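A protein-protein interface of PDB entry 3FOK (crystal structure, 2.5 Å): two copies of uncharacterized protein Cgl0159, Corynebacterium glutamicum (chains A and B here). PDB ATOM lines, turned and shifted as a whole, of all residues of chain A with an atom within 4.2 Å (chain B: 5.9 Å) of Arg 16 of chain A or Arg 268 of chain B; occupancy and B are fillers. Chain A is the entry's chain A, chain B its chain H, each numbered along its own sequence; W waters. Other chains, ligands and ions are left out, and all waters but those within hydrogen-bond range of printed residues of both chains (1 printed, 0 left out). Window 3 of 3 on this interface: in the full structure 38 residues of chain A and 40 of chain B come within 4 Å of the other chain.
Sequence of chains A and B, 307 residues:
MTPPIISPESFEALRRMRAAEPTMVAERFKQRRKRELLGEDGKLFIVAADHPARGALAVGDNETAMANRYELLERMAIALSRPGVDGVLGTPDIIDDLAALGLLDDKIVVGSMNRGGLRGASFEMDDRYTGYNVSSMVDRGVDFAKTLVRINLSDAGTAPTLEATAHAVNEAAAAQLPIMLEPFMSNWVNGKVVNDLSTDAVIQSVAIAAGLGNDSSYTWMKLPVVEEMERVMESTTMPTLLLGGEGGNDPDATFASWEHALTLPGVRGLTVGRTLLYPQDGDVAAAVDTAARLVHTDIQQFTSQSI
OE2 of Glu 12 of chain A lies within salt-bridge range of NH2 of Arg 15 of chain A, 2.5 Å away. OE1 of Glu 12 of chain A lies within salt-bridge range of NH2 of Arg 16 of chain A, at 2.8 Å. O of Gly 42 of chain B sits at hydrogen-bond distance from NH1 of Arg 268 of chain B, at 3.0 Å. The backbone NH of Leu 44 of chain B sits at hydrogen-bond distance from the backbone carbonyl oxygen of Arg 268 of chain B (2.8 Å). The backbone carbonyl oxygen of Gly 266 of chain B is in hydrogen-bond range of the backbone NH of Thr 240 of chain B (3.1 Å). The backbone NH of Arg 268 of chain B is in hydrogen-bond range of the backbone carbonyl oxygen of Thr 240 of chain B (2.7 Å).
CD2 of Leu 14 of chain A touches CG2 of Thr 237 of chain B, at 3.99 Å. Thr 237 of chain B touches Arg 15 of chain A (O to CG, 3.5 Å). Arg 15 of chain A touches Gly 266 of chain B. Arg 268 of chain B touches Arg 16 of chain A. Thr 237 of chain B touches Arg 18 of chain A. Arg 18 of chain A touches Pro 239 of chain B (CB to CD, 3.99 Å). Leu 38 of chain B touches Ala 19 of chain A (CD1 to O, 3.9 Å). Ala 19 of chain A touches Arg 268 of chain B.
Arg 16 of chain A touches just one residue of chain B: Arg 268 (3.9 Å). Arg 268 of chain B touches two residues of chain A. Printed residues of chain B within 4 Å of Leu 14 of chain A: Thr 237. Of the printed residues of chain A, Leu 38 of chain B touches Ala 19. Printed residues of chain A within 4 Å of Pro 239 of chain B: Arg 18. Ala 13 of chain A touches none of the printed residues of chain B. Asp 41 of chain B touches none of the printed residues of chain A. The nearest residue of chain B that does not touch Arg 16 of chain A is Thr 237 of chain B (5.8 Å). The nearest printed residue of chain A that does not touch Arg 268 of chain B is Arg 15 of chain A (4.8 Å). The nearest printed residue of chain B that does not touch Arg 15 of chain A is Arg 268 of chain B (4.8 Å).
Printed residues of chain B that touch a printed residue of chain A: Leu 38, Thr 237, Pro 239, Gly 266 and Arg 268. Of the 9 printed residues of chain A, 5 touch a printed residue of chain B. Hydrophobic or aromatic side chains of chain A within 4 Å of the printed part of chain B: Leu 14 and Ala 19. Along chain A the printed residues that touch a printed residue of chain B span positions 14 to 19.
No position is printed for both chains.
Water W1 bridges O of Thr 237 of chain B and O of Arg 15 of chain A.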
ATOM      1  N   GLU A  12     -12.452  -0.672 -10.186  1.00  0.00           N
ATOM      2  CA  GLU A  12     -11.319  -0.956  -9.322  1.00  0.00           C
ATOM      3  C   GLU A  12     -11.178   0.202  -8.340  1.00  0.00           C
ATOM      4  O   GLU A  12     -10.879   0.000  -7.167  1.00  0.00           O
ATOM      5  CB  GLU A  12     -10.027  -1.108 -10.132  1.00  0.00           C
ATOM      6  CG  GLU A  12      -8.828  -1.446  -9.267  1.00  0.00           C
ATOM      7  CD  GLU A  12      -9.018  -2.750  -8.509  1.00  0.00           C
ATOM      8  OE1 GLU A  12      -8.360  -2.939  -7.462  1.00  0.00           O
ATOM      9  OE2 GLU A  12      -9.819  -3.595  -8.969  1.00  0.00           O
ATOM     10  N   ALA A  13     -11.407   1.416  -8.828  1.00  0.00           N
ATOM     11  CA  ALA A  13     -11.314   2.610  -7.999  1.00  0.00           C
ATOM     12  C   ALA A  13     -12.430   2.635  -6.954  1.00  0.00           C
ATOM     13  O   ALA A  13     -12.193   3.003  -5.803  1.00  0.00           O
ATOM     14  CB  ALA A  13     -11.384   3.857  -8.873  1.00  0.00           C
ATOM     15  N   LEU A  14     -13.642   2.250  -7.357  1.00  0.00           N
ATOM     16  CA  LEU A  14     -14.793   2.218  -6.451  1.00  0.00           C
ATOM     17  C   LEU A  14     -14.548   1.242  -5.310  1.00  0.00           C
ATOM     18  O   LEU A  14     -14.655   1.605  -4.144  1.00  0.00           O
ATOM     19  CB  LEU A  14     -16.063   1.815  -7.214  1.00  0.00           C
ATOM     20  CG  LEU A  14     -17.333   1.412  -6.444  1.00  0.00           C
ATOM     21  CD1 LEU A  14     -17.820   2.543  -5.550  1.00  0.00           C
ATOM     22  CD2 LEU A  14     -18.417   1.038  -7.443  1.00  0.00           C
ATOM     23  N   ARG A  15     -14.228  -0.002  -5.653  1.00  0.00           N
ATOM     24  CA  ARG A  15     -13.951  -1.019  -4.642  1.00  0.00           C
ATOM     25  C   ARG A  15     -12.814  -0.530  -3.769  1.00  0.00           C
ATOM     26  O   ARG A  15     -12.880  -0.568  -2.540  1.00  0.00           O
ATOM     27  CB  ARG A  15     -13.510  -2.338  -5.285  1.00  0.00           C
ATOM     28  CG  ARG A  15     -14.599  -3.170  -5.922  1.00  0.00           C
ATOM     29  CD  ARG A  15     -14.063  -4.570  -6.208  1.00  0.00           C
ATOM     30  NE  ARG A  15     -12.973  -4.565  -7.179  1.00  0.00           N
ATOM     31  CZ  ARG A  15     -13.141  -4.706  -8.489  1.00  0.00           C
ATOM     32  NH1 ARG A  15     -14.357  -4.865  -8.990  1.00  0.00           N
ATOM     33  NH2 ARG A  15     -12.093  -4.687  -9.300  1.00  0.00           N
ATOM     34  N   ARG A  16     -11.761  -0.077  -4.434  1.00  0.00           N
ATOM     35  CA  ARG A  16     -10.572   0.411  -3.765  1.00  0.00           C
ATOM     36  C   ARG A  16     -10.873   1.633  -2.909  1.00  0.00           C
ATOM     37  O   ARG A  16     -10.187   1.894  -1.929  1.00  0.00           O
ATOM     38  CB  ARG A  16      -9.507   0.736  -4.807  1.00  0.00           C
ATOM     39  CG  ARG A  16      -8.140   1.000  -4.241  1.00  0.00           C
ATOM     40  CD  ARG A  16      -7.094   1.022  -5.343  1.00  0.00           C
ATOM     41  NE  ARG A  16      -6.923  -0.287  -5.972  1.00  0.00           N
ATOM     42  CZ  ARG A  16      -5.840  -0.636  -6.660  1.00  0.00           C
ATOM     43  NH1 ARG A  16      -4.839   0.226  -6.805  1.00  0.00           N
ATOM     44  NH2 ARG A  16      -5.749  -1.847  -7.196  1.00  0.00           N
ATOM     45  N   MET A  17     -11.912   2.377  -3.268  1.00  0.00           N
ATOM     46  CA  MET A  17     -12.263   3.563  -2.498  1.00  0.00           C
ATOM     47  C   MET A  17     -12.938   3.160  -1.191  1.00  0.00           C
ATOM     48  O   MET A  17     -12.510   3.572  -0.113  1.00  0.00           O
ATOM     49  CB  MET A  17     -13.198   4.477  -3.290  1.00  0.00           C
ATOM     50  CG  MET A  17     -13.394   5.829  -2.627  1.00  0.00           C
ATOM     51  SD  MET A  17     -14.838   6.885  -3.365  1.00  0.00           S
ATOM     52  CE  MET A  17     -14.033   7.374  -5.060  1.00  0.00           C
ATOM     53  N   ARG A  18     -13.991   2.354  -1.298  1.00  0.00           N
ATOM     54  CA  ARG A  18     -14.730   1.885  -0.132  1.00  0.00           C
ATOM     55  C   ARG A  18     -13.799   1.265   0.903  1.00  0.00           C
ATOM     56  O   ARG A  18     -14.009   1.400   2.112  1.00  0.00           O
ATOM     57  CB  ARG A  18     -15.767   0.842  -0.546  1.00  0.00           C
ATOM     58  CG  ARG A  18     -17.009   1.394  -1.225  1.00  0.00           C
ATOM     59  CD  ARG A  18     -17.899   0.250  -1.699  1.00  0.00           C
ATOM     60  NE  ARG A  18     -19.305   0.631  -1.753  1.00  0.00           N
ATOM     61  CZ  ARG A  18     -20.050   0.887  -0.683  1.00  0.00           C
ATOM     62  NH1 ARG A  18     -19.522   0.803   0.533  1.00  0.00           N
ATOM     63  NH2 ARG A  18     -21.325   1.228  -0.828  1.00  0.00           N
ATOM     64  N   ALA A  19     -12.768   0.585   0.419  1.00  0.00           N
ATOM     65  CA  ALA A  19     -11.813  -0.074   1.294  1.00  0.00           C
ATOM     66  C   ALA A  19     -10.898   0.871   2.063  1.00  0.00           C
ATOM     67  O   ALA A  19     -10.896   0.871   3.292  1.00  0.00           O
ATOM     68  CB  ALA A  19     -10.975  -1.057   0.485  1.00  0.00           C
ATOM     69  N   ALA A  20     -10.131   1.682   1.337  1.00  0.00           N
ATOM     70  CA  ALA A  20      -9.165   2.584   1.962  1.00  0.00           C
ATOM     71  C   ALA A  20      -9.521   4.063   2.142  1.00  0.00           C
ATOM     72  O   ALA A  20      -8.974   4.716   3.033  1.00  0.00           O
ATOM     73  CB  ALA A  20      -7.838   2.471   1.231  1.00  0.00           C
ATOM     74  N   LEU B  38      -5.425  -0.882   7.039  1.00  0.00           N
ATOM     75  CA  LEU B  38      -4.809  -1.641   5.963  1.00  0.00           C
ATOM     76  C   LEU B  38      -3.315  -1.378   5.850  1.00  0.00           C
ATOM     77  O   LEU B  38      -2.868  -0.231   5.881  1.00  0.00           O
ATOM     78  CB  LEU B  38      -5.489  -1.315   4.636  1.00  0.00           C
ATOM     79  CG  LEU B  38      -6.974  -1.661   4.583  1.00  0.00           C
ATOM     80  CD1 LEU B  38      -7.563  -1.177   3.272  1.00  0.00           C
ATOM     81  CD2 LEU B  38      -7.155  -3.165   4.732  1.00  0.00           C
ATOM     82  N   ASP B  41       0.199  -3.948   1.706  1.00  0.00           N
ATOM     83  CA  ASP B  41      -0.362  -4.834   0.691  1.00  0.00           C
ATOM     84  C   ASP B  41      -1.889  -4.783   0.661  1.00  0.00           C
ATOM     85  O   ASP B  41      -2.531  -5.502  -0.105  1.00  0.00           O
ATOM     86  CB  ASP B  41       0.130  -6.272   0.911  1.00  0.00           C
ATOM     87  CG  ASP B  41      -0.565  -6.963   2.062  1.00  0.00           C
ATOM     88  OD1 ASP B  41      -0.887  -6.294   3.069  1.00  0.00           O
ATOM     89  OD2 ASP B  41      -0.777  -8.188   1.956  1.00  0.00           O
ATOM     90  N   GLY B  42      -2.462  -3.922   1.499  1.00  0.00           N
ATOM     91  CA  GLY B  42      -3.905  -3.760   1.542  1.00  0.00           C
ATOM     92  C   GLY B  42      -4.718  -4.964   1.973  1.00  0.00           C
ATOM     93  O   GLY B  42      -5.942  -4.958   1.838  1.00  0.00           O
ATOM     94  N   LYS B  43      -4.053  -5.997   2.486  1.00  0.00           N
ATOM     95  CA  LYS B  43      -4.748  -7.196   2.937  1.00  0.00           C
ATOM     96  C   LYS B  43      -4.901  -7.223   4.451  1.00  0.00           C
ATOM     97  O   LYS B  43      -4.166  -6.550   5.174  1.00  0.00           O
ATOM     98  CB  LYS B  43      -4.015  -8.452   2.470  1.00  0.00           C
ATOM     99  CG  LYS B  43      -4.468  -8.977   1.113  1.00  0.00           C
ATOM    100  CD  LYS B  43      -4.206  -7.994  -0.003  1.00  0.00           C
ATOM    101  CE  LYS B  43      -4.521  -8.606  -1.362  1.00  0.00           C
ATOM    102  NZ  LYS B  43      -5.953  -8.989  -1.491  1.00  0.00           N
ATOM    103  N   LEU B  44      -5.854  -8.017   4.927  1.00  0.00           N
ATOM    104  CA  LEU B  44      -6.121  -8.110   6.355  1.00  0.00           C
ATOM    105  C   LEU B  44      -6.357  -9.563   6.782  1.00  0.00           C
ATOM    106  O   LEU B  44      -7.065 -10.312   6.109  1.00  0.00           O
ATOM    107  CB  LEU B  44      -7.354  -7.258   6.674  1.00  0.00           C
ATOM    108  CG  LEU B  44      -7.575  -6.680   8.071  1.00  0.00           C
ATOM    109  CD1 LEU B  44      -6.440  -5.741   8.440  1.00  0.00           C
ATOM    110  CD2 LEU B  44      -8.906  -5.926   8.081  1.00  0.00           C
ATOM    111  N   PHE B  45      -5.748  -9.957   7.895  1.00  0.00           N
ATOM    112  CA  PHE B  45      -5.904 -11.308   8.433  1.00  0.00           C
ATOM    113  C   PHE B  45      -6.240 -11.191   9.917  1.00  0.00           C
ATOM    114  O   PHE B  45      -5.422 -10.744  10.721  1.00  0.00           O
ATOM    115  CB  PHE B  45      -4.615 -12.115   8.232  1.00  0.00           C
ATOM    116  CG  PHE B  45      -4.611 -13.459   8.920  1.00  0.00           C
ATOM    117  CD1 PHE B  45      -5.784 -14.198   9.064  1.00  0.00           C
ATOM    118  CD2 PHE B  45      -3.421 -14.001   9.402  1.00  0.00           C
ATOM    119  CE1 PHE B  45      -5.767 -15.454   9.680  1.00  0.00           C
ATOM    120  CE2 PHE B  45      -3.396 -15.251  10.014  1.00  0.00           C
ATOM    121  CZ  PHE B  45      -4.570 -15.978  10.154  1.00  0.00           C
ATOM    122  N   TRP B 220     -18.414  -3.634   5.497  1.00  0.00           N
ATOM    123  CA  TRP B 220     -17.652  -4.711   4.887  1.00  0.00           C
ATOM    124  C   TRP B 220     -18.500  -5.970   4.944  1.00  0.00           C
ATOM    125  O   TRP B 220     -19.510  -6.019   5.641  1.00  0.00           O
ATOM    126  CB  TRP B 220     -16.362  -4.967   5.668  1.00  0.00           C
ATOM    127  CG  TRP B 220     -15.312  -3.920   5.521  1.00  0.00           C
ATOM    128  CD1 TRP B 220     -15.457  -2.575   5.706  1.00  0.00           C
ATOM    129  CD2 TRP B 220     -13.938  -4.132   5.179  1.00  0.00           C
ATOM    130  NE1 TRP B 220     -14.255  -1.935   5.499  1.00  0.00           N
ATOM    131  CE2 TRP B 220     -13.306  -2.868   5.174  1.00  0.00           C
ATOM    132  CE3 TRP B 220     -13.174  -5.270   4.876  1.00  0.00           C
ATOM    133  CZ2 TRP B 220     -11.949  -2.707   4.877  1.00  0.00           C
ATOM    134  CZ3 TRP B 220     -11.821  -5.109   4.581  1.00  0.00           C
ATOM    135  CH2 TRP B 220     -11.224  -3.838   4.584  1.00  0.00           C
ATOM    136  N   THR B 237     -19.652  -4.587  -4.256  1.00  0.00           N
ATOM    137  CA  THR B 237     -18.485  -3.798  -4.586  1.00  0.00           C
ATOM    138  C   THR B 237     -17.775  -3.523  -3.269  1.00  0.00           C
ATOM    139  O   THR B 237     -16.753  -2.837  -3.228  1.00  0.00           O
ATOM    140  CB  THR B 237     -18.906  -2.463  -5.202  1.00  0.00           C
ATOM    141  OG1 THR B 237     -19.837  -1.816  -4.327  1.00  0.00           O
ATOM    142  CG2 THR B 237     -19.566  -2.682  -6.552  1.00  0.00           C
ATOM    143  N   PRO B 239     -15.702  -4.206   0.356  1.00  0.00           N
ATOM    144  CA  PRO B 239     -14.531  -4.952   0.818  1.00  0.00           C
ATOM    145  C   PRO B 239     -15.012  -6.200   1.545  1.00  0.00           C
ATOM    146  O   PRO B 239     -15.884  -6.128   2.415  1.00  0.00           O
ATOM    147  CB  PRO B 239     -13.819  -3.949   1.729  1.00  0.00           C
ATOM    148  CG  PRO B 239     -14.925  -3.046   2.191  1.00  0.00           C
ATOM    149  CD  PRO B 239     -15.732  -2.858   0.947  1.00  0.00           C
ATOM    150  N   THR B 240     -14.445  -7.343   1.177  1.00  0.00           N
ATOM    151  CA  THR B 240     -14.857  -8.607   1.761  1.00  0.00           C
ATOM    152  C   THR B 240     -13.743  -9.381   2.450  1.00  0.00           C
ATOM    153  O   THR B 240     -12.591  -9.362   2.023  1.00  0.00           O
ATOM    154  CB  THR B 240     -15.485  -9.509   0.674  1.00  0.00           C
ATOM    155  OG1 THR B 240     -16.631  -8.854   0.118  1.00  0.00           O
ATOM    156  CG2 THR B 240     -15.907 -10.850   1.254  1.00  0.00           C
ATOM    157  N   LEU B 241     -14.107 -10.059   3.532  1.00  0.00           N
ATOM    158  CA  LEU B 241     -13.179 -10.883   4.292  1.00  0.00           C
ATOM    159  C   LEU B 241     -13.803 -12.271   4.338  1.00  0.00           C
ATOM    160  O   LEU B 241     -15.018 -12.410   4.486  1.00  0.00           O
ATOM    161  CB  LEU B 241     -12.997 -10.329   5.705  1.00  0.00           C
ATOM    162  CG  LEU B 241     -12.259  -8.988   5.776  1.00  0.00           C
ATOM    163  CD1 LEU B 241     -12.286  -8.455   7.198  1.00  0.00           C
ATOM    164  CD2 LEU B 241     -10.832  -9.163   5.292  1.00  0.00           C
ATOM    165  N   LEU B 262      -9.323 -15.804  -2.436  1.00  0.00           N
ATOM    166  CA  LEU B 262      -8.491 -14.668  -2.065  1.00  0.00           C
ATOM    167  C   LEU B 262      -8.041 -13.843  -3.270  1.00  0.00           C
ATOM    168  O   LEU B 262      -7.617 -12.696  -3.118  1.00  0.00           O
ATOM    169  CB  LEU B 262      -7.273 -15.174  -1.289  1.00  0.00           C
ATOM    170  CG  LEU B 262      -7.002 -14.654   0.125  1.00  0.00           C
ATOM    171  CD1 LEU B 262      -8.304 -14.366   0.857  1.00  0.00           C
ATOM    172  CD2 LEU B 262      -6.180 -15.690   0.876  1.00  0.00           C
ATOM    173  N   GLY B 266     -12.293  -7.534  -4.946  1.00  0.00           N
ATOM    174  CA  GLY B 266     -12.881  -7.058  -3.710  1.00  0.00           C
ATOM    175  C   GLY B 266     -12.500  -7.796  -2.442  1.00  0.00           C
ATOM    176  O   GLY B 266     -12.656  -7.250  -1.349  1.00  0.00           O
ATOM    177  N   VAL B 267     -12.022  -9.031  -2.564  1.00  0.00           N
ATOM    178  CA  VAL B 267     -11.629  -9.786  -1.379  1.00  0.00           C
ATOM    179  C   VAL B 267     -10.367  -9.160  -0.793  1.00  0.00           C
ATOM    180  O   VAL B 267      -9.362  -8.995  -1.483  1.00  0.00           O
ATOM    181  CB  VAL B 267     -11.380 -11.269  -1.713  1.00  0.00           C
ATOM    182  CG1 VAL B 267     -10.952 -12.021  -0.466  1.00  0.00           C
ATOM    183  CG2 VAL B 267     -12.651 -11.883  -2.285  1.00  0.00           C
ATOM    184  N   ARG B 268     -10.433  -8.808   0.485  1.00  0.00           N
ATOM    185  CA  ARG B 268      -9.323  -8.159   1.173  1.00  0.00           C
ATOM    186  C   ARG B 268      -8.598  -8.999   2.218  1.00  0.00           C
ATOM    187  O   ARG B 268      -7.645  -8.527   2.839  1.00  0.00           O
ATOM    188  CB  ARG B 268      -9.823  -6.873   1.834  1.00  0.00           C
ATOM    189  CG  ARG B 268     -10.100  -5.746   0.856  1.00  0.00           C
ATOM    190  CD  ARG B 268      -8.817  -5.029   0.513  1.00  0.00           C
ATOM    191  NE  ARG B 268      -9.014  -3.994  -0.492  1.00  0.00           N
ATOM    192  CZ  ARG B 268      -8.159  -3.002  -0.710  1.00  0.00           C
ATOM    193  NH1 ARG B 268      -7.052  -2.912   0.015  1.00  0.00           N
ATOM    194  NH2 ARG B 268      -8.404  -2.103  -1.655  1.00  0.00           N
ATOM    195  N   GLY B 269      -9.046 -10.230   2.434  1.00  0.00           N
ATOM    196  CA  GLY B 269      -8.378 -11.055   3.422  1.00  0.00           C
ATOM    197  C   GLY B 269      -9.208 -12.104   4.131  1.00  0.00           C
ATOM    198  O   GLY B 269     -10.209 -12.592   3.608  1.00  0.00           O
ATOM    199  N   LEU B 270      -8.778 -12.437   5.344  1.00  0.00           N
ATOM    200  CA  LEU B 270      -9.423 -13.456   6.165  1.00  0.00           C
ATOM    201  C   LEU B 270      -9.797 -13.002   7.577  1.00  0.00           C
ATOM    202  O   LEU B 270      -9.161 -12.121   8.159  1.00  0.00           O
ATOM    203  CB  LEU B 270      -8.492 -14.664   6.293  1.00  0.00           C
ATOM    204  CG  LEU B 270      -8.558 -15.891   5.377  1.00  0.00           C
ATOM    205  CD1 LEU B 270      -8.921 -15.512   3.958  1.00  0.00           C
ATOM    206  CD2 LEU B 270      -7.210 -16.594   5.432  1.00  0.00           C
ATOM    207  N   VAL B 295      -2.540 -14.896   2.970  1.00  0.00           N
ATOM    208  CA  VAL B 295      -3.103 -13.548   2.964  1.00  0.00           C
ATOM    209  C   VAL B 295      -2.037 -12.503   2.644  1.00  0.00           C
ATOM    210  O   VAL B 295      -2.317 -11.503   1.984  1.00  0.00           O
ATOM    211  CB  VAL B 295      -3.751 -13.202   4.322  1.00  0.00           C
ATOM    212  CG1 VAL B 295      -4.138 -11.732   4.358  1.00  0.00           C
ATOM    213  CG2 VAL B 295      -4.983 -14.064   4.540  1.00  0.00           C
HETATM  214  O   HOH W   1     -14.505  -3.086  -1.901  1.00  0.00           O
